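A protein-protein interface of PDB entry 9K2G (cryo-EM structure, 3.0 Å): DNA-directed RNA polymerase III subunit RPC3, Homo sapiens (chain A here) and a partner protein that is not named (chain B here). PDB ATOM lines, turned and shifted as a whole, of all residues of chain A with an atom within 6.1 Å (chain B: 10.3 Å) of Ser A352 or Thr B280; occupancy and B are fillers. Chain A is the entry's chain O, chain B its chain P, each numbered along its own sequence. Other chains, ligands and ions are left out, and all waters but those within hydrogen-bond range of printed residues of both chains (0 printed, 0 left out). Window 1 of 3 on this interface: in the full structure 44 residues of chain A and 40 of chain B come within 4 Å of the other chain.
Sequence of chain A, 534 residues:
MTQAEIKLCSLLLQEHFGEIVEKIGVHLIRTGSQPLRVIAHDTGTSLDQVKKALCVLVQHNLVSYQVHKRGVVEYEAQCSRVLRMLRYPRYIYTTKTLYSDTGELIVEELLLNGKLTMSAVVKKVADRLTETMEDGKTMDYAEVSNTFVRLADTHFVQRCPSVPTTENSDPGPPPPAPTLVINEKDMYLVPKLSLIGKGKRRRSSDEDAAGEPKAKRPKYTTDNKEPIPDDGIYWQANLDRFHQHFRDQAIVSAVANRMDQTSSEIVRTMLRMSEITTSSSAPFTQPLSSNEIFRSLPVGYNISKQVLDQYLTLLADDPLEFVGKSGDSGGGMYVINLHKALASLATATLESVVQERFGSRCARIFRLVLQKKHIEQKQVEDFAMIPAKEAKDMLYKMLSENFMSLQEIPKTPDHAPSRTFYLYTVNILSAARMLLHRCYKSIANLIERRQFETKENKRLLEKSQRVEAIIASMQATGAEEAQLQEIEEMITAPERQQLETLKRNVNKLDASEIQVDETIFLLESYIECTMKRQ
Ser A352 touches two residues of chain B. Of chain A, only Thr A349, Ser A352 and Thr A519 come within 4 Å of Thr B280. Thr A349 touches just these residues of chain B: Ile B277 (3.6 Å) and Thr B280 (3.6 Å). Glu A356 touches two residues of chain B. Printed residues of chain B within 4 Å of Glu A518: Gly B281. Of the printed residues of chain A, Pro B279 touches Ser A352 (3.3 Å). Ile B276 touches none of the printed residues of chain A. The nearest printed residue of chain B that does not touch Arg A357 is Val B283 (5.2 Å).
Among the printed residues, merely in contact across the chains: Ala A348 with Ile B277 (3.9 Å), Thr A349 with Ile B277 (3.6 Å), Thr A349 with Thr B280 (3.6 Å), Ser A352 with Pro B279 (3.3 Å), Val A353 with Leu B282 (3.8 Å), Val A353 with Val B283 (3.6 Å), Glu A356 with Val B283 (3.6 Å), Glu A356 with Leu B289 (3.9 Å), Arg A357 with Gly B288 (3.9 Å), Arg A357 with Leu B289 (3.8 Å), Arg A367 with Gly B246 (3.7 Å), Gln A515 with Gly B281 (3.5 Å), Gln A515 with Arg B284 (3.2 Å), Glu A518 with Gly B281 (3.7 Å) and Thr A519 with Thr B280 (3.3 Å).
Hydrophobic or aromatic side chains of chain A that line the printed part of chain B: Ala A348 and Val A353. Along chain A the printed residues that touch a printed residue of chain B span positions 348 to 519. Among the printed residues, 20 pairs touch across the chains.
The side-chain carboxylate (OE1) of Glu A351 lies within salt-bridge range of the guanidinium group (NE) of Arg A367 (2.9 Å). NH2 of Arg A367 is in hydrogen-bond range of OE1 of Gln A355. The guanidinium group (NH2) of Arg B284 lies close to the backbone carbonyl oxygen (O) of Pro B279 (3.2 Å). The guanidinium group (NH1) of Arg B284 is in hydrogen-bond range of the backbone carbonyl oxygen (O) of Thr B280, 3.1 Å away.
The side-chain hydroxyl of Ser A352 lies within hydrogen-bond range of the backbone NH of Thr B280, 3.5 Å away. The guanidinium group (NH1) of Arg A367 lies close to the backbone carbonyl oxygen (O) of Tyr B244 (3.4 Å). The guanidinium group (NH1) of Arg A367 is in salt-bridge range of the side-chain carboxylate (OD1) of Asp B245 (3.9 Å). OG1 of Thr A519 lies within hydrogen-bond range of N of Gly B281. The backbone NH (N) of Leu B282 is in hydrogen-bond range of the side-chain hydroxyl (OG1) of Thr A519, 3.4 Å away.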
ATOM      1  N   THR A 347     -10.642  32.262  22.846  1.00  0.00           N
ATOM      2  CA  THR A 347     -11.939  31.996  23.465  1.00  0.00           C
ATOM      3  C   THR A 347     -12.091  30.524  23.811  1.00  0.00           C
ATOM      4  O   THR A 347     -12.581  30.180  24.897  1.00  0.00           O
ATOM      5  CB  THR A 347     -13.055  32.447  22.522  1.00  0.00           C
ATOM      6  OG1 THR A 347     -13.127  33.880  22.494  1.00  0.00           O
ATOM      7  CG2 THR A 347     -14.395  31.880  22.958  1.00  0.00           C
ATOM      8  N   ALA A 348     -11.678  29.636  22.905  1.00  0.00           N
ATOM      9  CA  ALA A 348     -11.751  28.203  23.178  1.00  0.00           C
ATOM     10  C   ALA A 348     -10.861  27.816  24.352  1.00  0.00           C
ATOM     11  O   ALA A 348     -11.257  27.014  25.201  1.00  0.00           O
ATOM     12  CB  ALA A 348     -11.364  27.412  21.928  1.00  0.00           C
ATOM     13  N   THR A 349      -9.654  28.381  24.418  1.00  0.00           N
ATOM     14  CA  THR A 349      -8.769  28.113  25.546  1.00  0.00           C
ATOM     15  C   THR A 349      -9.385  28.579  26.862  1.00  0.00           C
ATOM     16  O   THR A 349      -9.338  27.860  27.873  1.00  0.00           O
ATOM     17  CB  THR A 349      -7.411  28.786  25.320  1.00  0.00           C
ATOM     18  OG1 THR A 349      -6.677  28.067  24.318  1.00  0.00           O
ATOM     19  CG2 THR A 349      -6.599  28.838  26.608  1.00  0.00           C
ATOM     20  N   LEU A 350      -9.976  29.775  26.862  1.00  0.00           N
ATOM     21  CA  LEU A 350     -10.584  30.306  28.075  1.00  0.00           C
ATOM     22  C   LEU A 350     -11.766  29.452  28.517  1.00  0.00           C
ATOM     23  O   LEU A 350     -11.912  29.138  29.707  1.00  0.00           O
ATOM     24  CB  LEU A 350     -11.014  31.756  27.842  1.00  0.00           C
ATOM     25  CG  LEU A 350     -11.158  32.656  29.067  1.00  0.00           C
ATOM     26  CD1 LEU A 350      -9.868  32.668  29.874  1.00  0.00           C
ATOM     27  CD2 LEU A 350     -11.531  34.061  28.633  1.00  0.00           C
ATOM     28  N   GLU A 351     -12.620  29.051  27.572  1.00  0.00           N
ATOM     29  CA  GLU A 351     -13.755  28.209  27.935  1.00  0.00           C
ATOM     30  C   GLU A 351     -13.293  26.839  28.411  1.00  0.00           C
ATOM     31  O   GLU A 351     -13.896  26.273  29.327  1.00  0.00           O
ATOM     32  CB  GLU A 351     -14.734  28.091  26.765  1.00  0.00           C
ATOM     33  CG  GLU A 351     -14.360  27.074  25.697  1.00  0.00           C
ATOM     34  CD  GLU A 351     -15.428  26.919  24.635  1.00  0.00           C
ATOM     35  OE1 GLU A 351     -16.246  27.852  24.472  1.00  0.00           O
ATOM     36  OE2 GLU A 351     -15.458  25.864  23.968  1.00  0.00           O
ATOM     37  N   SER A 352     -12.216  26.303  27.829  1.00  0.00           N
ATOM     38  CA  SER A 352     -11.702  25.010  28.263  1.00  0.00           C
ATOM     39  C   SER A 352     -11.153  25.076  29.680  1.00  0.00           C
ATOM     40  O   SER A 352     -11.412  24.177  30.491  1.00  0.00           O
ATOM     41  CB  SER A 352     -10.628  24.523  27.296  1.00  0.00           C
ATOM     42  OG  SER A 352     -10.060  23.303  27.741  1.00  0.00           O
ATOM     43  N   VAL A 353     -10.394  26.127  30.003  1.00  0.00           N
ATOM     44  CA  VAL A 353      -9.849  26.224  31.355  1.00  0.00           C
ATOM     45  C   VAL A 353     -10.965  26.463  32.366  1.00  0.00           C
ATOM     46  O   VAL A 353     -10.947  25.904  33.470  1.00  0.00           O
ATOM     47  CB  VAL A 353      -8.745  27.300  31.437  1.00  0.00           C
ATOM     48  CG1 VAL A 353      -9.269  28.677  31.083  1.00  0.00           C
ATOM     49  CG2 VAL A 353      -8.117  27.316  32.829  1.00  0.00           C
ATOM     50  N   VAL A 354     -11.975  27.261  31.999  1.00  0.00           N
ATOM     51  CA  VAL A 354     -13.120  27.453  32.888  1.00  0.00           C
ATOM     52  C   VAL A 354     -13.846  26.132  33.120  1.00  0.00           C
ATOM     53  O   VAL A 354     -14.203  25.794  34.257  1.00  0.00           O
ATOM     54  CB  VAL A 354     -14.063  28.534  32.322  1.00  0.00           C
ATOM     55  CG1 VAL A 354     -15.414  28.474  33.019  1.00  0.00           C
ATOM     56  CG2 VAL A 354     -13.445  29.916  32.486  1.00  0.00           C
ATOM     57  N   GLN A 355     -14.065  25.362  32.052  1.00  0.00           N
ATOM     58  CA  GLN A 355     -14.758  24.088  32.180  1.00  0.00           C
ATOM     59  C   GLN A 355     -13.979  23.113  33.057  1.00  0.00           C
ATOM     60  O   GLN A 355     -14.563  22.441  33.920  1.00  0.00           O
ATOM     61  CB  GLN A 355     -15.004  23.478  30.801  1.00  0.00           C
ATOM     62  CG  GLN A 355     -15.531  22.054  30.841  1.00  0.00           C
ATOM     63  CD  GLN A 355     -16.266  21.673  29.571  1.00  0.00           C
ATOM     64  OE1 GLN A 355     -16.529  22.515  28.714  1.00  0.00           O
ATOM     65  NE2 GLN A 355     -16.607  20.396  29.444  1.00  0.00           N
ATOM     66  N   GLU A 356     -12.668  23.020  32.860  1.00  0.00           N
ATOM     67  CA  GLU A 356     -11.875  22.078  33.638  1.00  0.00           C
ATOM     68  C   GLU A 356     -11.648  22.532  35.073  1.00  0.00           C
ATOM     69  O   GLU A 356     -11.359  21.692  35.932  1.00  0.00           O
ATOM     70  CB  GLU A 356     -10.533  21.815  32.955  1.00  0.00           C
ATOM     71  CG  GLU A 356     -10.607  20.782  31.849  1.00  0.00           C
ATOM     72  CD  GLU A 356     -11.171  19.457  32.335  1.00  0.00           C
ATOM     73  OE1 GLU A 356     -10.805  19.029  33.448  1.00  0.00           O
ATOM     74  OE2 GLU A 356     -11.983  18.856  31.607  1.00  0.00           O
ATOM     75  N   ARG A 357     -11.772  23.827  35.359  1.00  0.00           N
ATOM     76  CA  ARG A 357     -11.560  24.293  36.721  1.00  0.00           C
ATOM     77  C   ARG A 357     -12.846  24.381  37.534  1.00  0.00           C
ATOM     78  O   ARG A 357     -12.796  24.292  38.766  1.00  0.00           O
ATOM     79  CB  ARG A 357     -10.865  25.658  36.709  1.00  0.00           C
ATOM     80  CG  ARG A 357     -10.276  26.067  38.046  1.00  0.00           C
ATOM     81  CD  ARG A 357      -9.687  27.458  37.988  1.00  0.00           C
ATOM     82  NE  ARG A 357      -9.447  27.995  39.324  1.00  0.00           N
ATOM     83  CZ  ARG A 357      -9.113  29.253  39.574  1.00  0.00           C
ATOM     84  NH1 ARG A 357      -8.960  30.136  38.600  1.00  0.00           N
ATOM     85  NH2 ARG A 357      -8.930  29.638  40.833  1.00  0.00           N
ATOM     86  N   PHE A 366     -20.445  30.549  31.486  1.00  0.00           N
ATOM     87  CA  PHE A 366     -19.403  31.381  30.881  1.00  0.00           C
ATOM     88  C   PHE A 366     -19.680  31.624  29.403  1.00  0.00           C
ATOM     89  O   PHE A 366     -19.571  32.752  28.914  1.00  0.00           O
ATOM     90  CB  PHE A 366     -18.039  30.717  31.082  1.00  0.00           C
ATOM     91  CG  PHE A 366     -16.904  31.432  30.408  1.00  0.00           C
ATOM     92  CD1 PHE A 366     -16.458  32.653  30.873  1.00  0.00           C
ATOM     93  CD2 PHE A 366     -16.269  30.865  29.311  1.00  0.00           C
ATOM     94  CE1 PHE A 366     -15.407  33.311  30.257  1.00  0.00           C
ATOM     95  CE2 PHE A 366     -15.219  31.515  28.692  1.00  0.00           C
ATOM     96  CZ  PHE A 366     -14.788  32.738  29.163  1.00  0.00           C
ATOM     97  N   ARG A 367     -20.054  30.571  28.673  1.00  0.00           N
ATOM     98  CA  ARG A 367     -20.365  30.739  27.253  1.00  0.00           C
ATOM     99  C   ARG A 367     -21.621  31.579  27.060  1.00  0.00           C
ATOM    100  O   ARG A 367     -21.703  32.370  26.111  1.00  0.00           O
ATOM    101  CB  ARG A 367     -20.518  29.377  26.581  1.00  0.00           C
ATOM    102  CG  ARG A 367     -19.245  28.553  26.532  1.00  0.00           C
ATOM    103  CD  ARG A 367     -19.421  27.319  25.663  1.00  0.00           C
ATOM    104  NE  ARG A 367     -18.346  26.360  25.851  1.00  0.00           N
ATOM    105  CZ  ARG A 367     -18.338  25.427  26.798  1.00  0.00           C
ATOM    106  NH1 ARG A 367     -19.332  25.308  27.658  1.00  0.00           N
ATOM    107  NH2 ARG A 367     -17.304  24.592  26.874  1.00  0.00           N
ATOM    108  N   GLN A 515       3.839  21.193  27.925  1.00  0.00           N
ATOM    109  CA  GLN A 515       2.496  21.298  27.358  1.00  0.00           C
ATOM    110  C   GLN A 515       1.784  22.588  27.756  1.00  0.00           C
ATOM    111  O   GLN A 515       0.937  23.073  26.999  1.00  0.00           O
ATOM    112  CB  GLN A 515       1.671  20.074  27.747  1.00  0.00           C
ATOM    113  CG  GLN A 515       2.186  18.789  27.110  1.00  0.00           C
ATOM    114  CD  GLN A 515       1.268  17.606  27.330  1.00  0.00           C
ATOM    115  OE1 GLN A 515       0.126  17.761  27.765  1.00  0.00           O
ATOM    116  NE2 GLN A 515       1.762  16.413  27.025  1.00  0.00           N
ATOM    117  N   GLU A 518       2.161  25.445  25.220  1.00  0.00           N
ATOM    118  CA  GLU A 518       1.237  25.611  24.098  1.00  0.00           C
ATOM    119  C   GLU A 518       0.143  26.620  24.426  1.00  0.00           C
ATOM    120  O   GLU A 518      -0.181  27.500  23.615  1.00  0.00           O
ATOM    121  CB  GLU A 518       0.638  24.256  23.720  1.00  0.00           C
ATOM    122  CG  GLU A 518      -0.503  24.324  22.720  1.00  0.00           C
ATOM    123  CD  GLU A 518      -1.865  24.299  23.387  1.00  0.00           C
ATOM    124  OE1 GLU A 518      -1.976  23.745  24.499  1.00  0.00           O
ATOM    125  OE2 GLU A 518      -2.823  24.844  22.799  1.00  0.00           O
ATOM    126  N   THR A 519      -0.443  26.513  25.624  1.00  0.00           N
ATOM    127  CA  THR A 519      -1.426  27.499  26.059  1.00  0.00           C
ATOM    128  C   THR A 519      -0.794  28.883  26.141  1.00  0.00           C
ATOM    129  O   THR A 519      -1.416  29.885  25.754  1.00  0.00           O
ATOM    130  CB  THR A 519      -2.005  27.099  27.416  1.00  0.00           C
ATOM    131  OG1 THR A 519      -2.549  25.773  27.335  1.00  0.00           O
ATOM    132  CG2 THR A 519      -3.102  28.065  27.840  1.00  0.00           C
ATOM    133  N   TYR B 244     -25.079  26.684  24.771  1.00  0.00           N
ATOM    134  CA  TYR B 244     -24.230  27.325  25.769  1.00  0.00           C
ATOM    135  C   TYR B 244     -23.275  26.341  26.423  1.00  0.00           C
ATOM    136  O   TYR B 244     -22.295  26.765  27.044  1.00  0.00           O
ATOM    137  CB  TYR B 244     -25.100  28.016  26.821  1.00  0.00           C
ATOM    138  CG  TYR B 244     -25.974  29.109  26.248  1.00  0.00           C
ATOM    139  CD1 TYR B 244     -25.538  29.887  25.187  1.00  0.00           C
ATOM    140  CD2 TYR B 244     -27.244  29.350  26.762  1.00  0.00           C
ATOM    141  CE1 TYR B 244     -26.336  30.882  24.653  1.00  0.00           C
ATOM    142  CE2 TYR B 244     -28.047  30.345  26.234  1.00  0.00           C
ATOM    143  CZ  TYR B 244     -27.589  31.107  25.180  1.00  0.00           C
ATOM    144  OH  TYR B 244     -28.385  32.096  24.652  1.00  0.00           O
ATOM    145  N   ASP B 245     -23.531  25.043  26.297  1.00  0.00           N
ATOM    146  CA  ASP B 245     -22.606  24.024  26.777  1.00  0.00           C
ATOM    147  C   ASP B 245     -21.465  23.767  25.798  1.00  0.00           C
ATOM    148  O   ASP B 245     -20.559  22.991  26.116  1.00  0.00           O
ATOM    149  CB  ASP B 245     -23.361  22.721  27.054  1.00  0.00           C
ATOM    150  CG  ASP B 245     -22.684  21.867  28.105  1.00  0.00           C
ATOM    151  OD1 ASP B 245     -21.637  22.292  28.639  1.00  0.00           O
ATOM    152  OD2 ASP B 245     -23.205  20.770  28.409  1.00  0.00           O
ATOM    153  N   GLY B 246     -21.488  24.399  24.621  1.00  0.00           N
ATOM    154  CA  GLY B 246     -20.416  24.248  23.658  1.00  0.00           C
ATOM    155  C   GLY B 246     -20.401  22.939  22.901  1.00  0.00           C
ATOM    156  O   GLY B 246     -19.351  22.551  22.387  1.00  0.00           O
ATOM    157  N   PRO B 275     -15.827  20.002  19.831  1.00  0.00           N
ATOM    158  CA  PRO B 275     -15.128  21.161  20.397  1.00  0.00           C
ATOM    159  C   PRO B 275     -13.964  21.593  19.522  1.00  0.00           C
ATOM    160  O   PRO B 275     -13.382  20.798  18.783  1.00  0.00           O
ATOM    161  CB  PRO B 275     -14.645  20.650  21.761  1.00  0.00           C
ATOM    162  CG  PRO B 275     -14.605  19.168  21.622  1.00  0.00           C
ATOM    163  CD  PRO B 275     -15.740  18.820  20.708  1.00  0.00           C
ATOM    164  N   ILE B 276     -13.634  22.884  19.615  1.00  0.00           N
ATOM    165  CA  ILE B 276     -12.587  23.452  18.768  1.00  0.00           C
ATOM    166  C   ILE B 276     -11.242  22.795  19.058  1.00  0.00           C
ATOM    167  O   ILE B 276     -10.544  22.341  18.146  1.00  0.00           O
ATOM    168  CB  ILE B 276     -12.517  24.978  18.954  1.00  0.00           C
ATOM    169  CG1 ILE B 276     -13.786  25.649  18.424  1.00  0.00           C
ATOM    170  CG2 ILE B 276     -11.278  25.547  18.272  1.00  0.00           C
ATOM    171  CD1 ILE B 276     -13.761  27.154  18.507  1.00  0.00           C
ATOM    172  N   ILE B 277     -10.864  22.730  20.333  1.00  0.00           N
ATOM    173  CA  ILE B 277      -9.559  22.199  20.727  1.00  0.00           C
ATOM    174  C   ILE B 277      -9.734  21.267  21.914  1.00  0.00           C
ATOM    175  O   ILE B 277     -10.706  21.373  22.677  1.00  0.00           O
ATOM    176  CB  ILE B 277      -8.562  23.318  21.079  1.00  0.00           C
ATOM    177  CG1 ILE B 277      -9.129  24.215  22.178  1.00  0.00           C
ATOM    178  CG2 ILE B 277      -8.198  24.125  19.845  1.00  0.00           C
ATOM    179  CD1 ILE B 277      -8.164  25.274  22.663  1.00  0.00           C
ATOM    180  N   PRO B 278      -8.807  20.331  22.090  1.00  0.00           N
ATOM    181  CA  PRO B 278      -8.780  19.532  23.319  1.00  0.00           C
ATOM    182  C   PRO B 278      -8.499  20.409  24.525  1.00  0.00           C
ATOM    183  O   PRO B 278      -8.179  21.601  24.367  1.00  0.00           O
ATOM    184  CB  PRO B 278      -7.636  18.537  23.069  1.00  0.00           C
ATOM    185  CG  PRO B 278      -7.502  18.475  21.588  1.00  0.00           C
ATOM    186  CD  PRO B 278      -7.827  19.854  21.101  1.00  0.00           C
ATOM    187  N   PRO B 279      -8.618  19.874  25.740  1.00  0.00           N
ATOM    188  CA  PRO B 279      -8.296  20.685  26.923  1.00  0.00           C
ATOM    189  C   PRO B 279      -6.872  21.217  26.853  1.00  0.00           C
ATOM    190  O   PRO B 279      -5.950  20.528  26.415  1.00  0.00           O
ATOM    191  CB  PRO B 279      -8.475  19.703  28.086  1.00  0.00           C
ATOM    192  CG  PRO B 279      -9.491  18.738  27.587  1.00  0.00           C
ATOM    193  CD  PRO B 279      -9.222  18.583  26.114  1.00  0.00           C
ATOM    194  N   THR B 280      -6.706  22.463  27.288  1.00  0.00           N
ATOM    195  CA  THR B 280      -5.433  23.149  27.156  1.00  0.00           C
ATOM    196  C   THR B 280      -4.397  22.551  28.110  1.00  0.00           C
ATOM    197  O   THR B 280      -4.718  21.785  29.022  1.00  0.00           O
ATOM    198  CB  THR B 280      -5.598  24.646  27.416  1.00  0.00           C
ATOM    199  OG1 THR B 280      -5.985  24.853  28.783  1.00  0.00           O
ATOM    200  CG2 THR B 280      -6.665  25.219  26.506  1.00  0.00           C
ATOM    201  N   GLY B 281      -3.137  22.914  27.880  1.00  0.00           N
ATOM    202  CA  GLY B 281      -2.065  22.407  28.717  1.00  0.00           C
ATOM    203  C   GLY B 281      -2.092  22.958  30.128  1.00  0.00           C
ATOM    204  O   GLY B 281      -1.583  22.325  31.056  1.00  0.00           O
ATOM    205  N   LEU B 282      -2.696  24.139  30.316  1.00  0.00           N
ATOM    206  CA  LEU B 282      -2.721  24.762  31.637  1.00  0.00           C
ATOM    207  C   LEU B 282      -3.477  23.908  32.644  1.00  0.00           C
ATOM    208  O   LEU B 282      -3.031  23.734  33.784  1.00  0.00           O
ATOM    209  CB  LEU B 282      -3.338  26.155  31.551  1.00  0.00           C
ATOM    210  CG  LEU B 282      -3.627  26.833  32.891  1.00  0.00           C
ATOM    211  CD1 LEU B 282      -2.341  27.058  33.680  1.00  0.00           C
ATOM    212  CD2 LEU B 282      -4.379  28.139  32.687  1.00  0.00           C
ATOM    213  N   VAL B 283      -4.632  23.363  32.248  1.00  0.00           N
ATOM    214  CA  VAL B 283      -5.431  22.550  33.159  1.00  0.00           C
ATOM    215  C   VAL B 283      -4.819  21.185  33.416  1.00  0.00           C
ATOM    216  O   VAL B 283      -5.286  20.468  34.308  1.00  0.00           O
ATOM    217  CB  VAL B 283      -6.866  22.383  32.632  1.00  0.00           C
ATOM    218  CG1 VAL B 283      -7.502  23.742  32.407  1.00  0.00           C
ATOM    219  CG2 VAL B 283      -6.873  21.564  31.353  1.00  0.00           C
ATOM    220  N   ARG B 284      -3.791  20.802  32.659  1.00  0.00           N
ATOM    221  CA  ARG B 284      -3.107  19.537  32.892  1.00  0.00           C
ATOM    222  C   ARG B 284      -2.086  19.619  34.022  1.00  0.00           C
ATOM    223  O   ARG B 284      -1.508  18.590  34.387  1.00  0.00           O
ATOM    224  CB  ARG B 284      -2.430  19.062  31.606  1.00  0.00           C
ATOM    225  CG  ARG B 284      -3.409  18.684  30.510  1.00  0.00           C
ATOM    226  CD  ARG B 284      -2.712  18.073  29.309  1.00  0.00           C
ATOM    227  NE  ARG B 284      -3.662  17.478  28.382  1.00  0.00           N
ATOM    228  CZ  ARG B 284      -4.263  18.137  27.400  1.00  0.00           C
ATOM    229  NH1 ARG B 284      -4.028  19.420  27.180  1.00  0.00           N
ATOM    230  NH2 ARG B 284      -5.122  17.491  26.614  1.00  0.00           N
ATOM    231  N   ALA B 285      -1.859  20.810  34.578  1.00  0.00           N
ATOM    232  CA  ALA B 285      -0.990  21.002  35.726  1.00  0.00           C
ATOM    233  C   ALA B 285      -1.813  21.390  36.950  1.00  0.00           C
ATOM    234  O   ALA B 285      -2.808  22.110  36.818  1.00  0.00           O
ATOM    235  CB  ALA B 285       0.058  22.087  35.456  1.00  0.00           C
ATOM    236  N   PRO B 286      -1.437  20.917  38.143  1.00  0.00           N
ATOM    237  CA  PRO B 286      -2.218  21.258  39.343  1.00  0.00           C
ATOM    238  C   PRO B 286      -2.291  22.748  39.624  1.00  0.00           C
ATOM    239  O   PRO B 286      -3.305  23.219  40.148  1.00  0.00           O
ATOM    240  CB  PRO B 286      -1.478  20.513  40.462  1.00  0.00           C
ATOM    241  CG  PRO B 286      -0.717  19.432  39.770  1.00  0.00           C
ATOM    242  CD  PRO B 286      -0.320  20.010  38.445  1.00  0.00           C
ATOM    243  N   GLY B 288      -2.705  25.086  37.582  1.00  0.00           N
ATOM    244  CA  GLY B 288      -3.781  25.656  36.796  1.00  0.00           C
ATOM    245  C   GLY B 288      -5.151  25.471  37.406  1.00  0.00           C
ATOM    246  O   GLY B 288      -6.074  26.218  37.070  1.00  0.00           O
ATOM    247  N   LEU B 289      -5.307  24.493  38.298  1.00  0.00           N
ATOM    248  CA  LEU B 289      -6.571  24.235  38.974  1.00  0.00           C
ATOM    249  C   LEU B 289      -6.498  24.480  40.477  1.00  0.00           C
ATOM    250  O   LEU B 289      -7.468  24.188  41.189  1.00  0.00           O
ATOM    251  CB  LEU B 289      -7.032  22.800  38.711  1.00  0.00           C
ATOM    252  CG  LEU B 289      -7.102  22.353  37.246  1.00  0.00           C
ATOM    253  CD1 LEU B 289      -7.681  20.955  37.139  1.00  0.00           C
ATOM    254  CD2 LEU B 289      -7.903  23.341  36.407  1.00  0.00           C
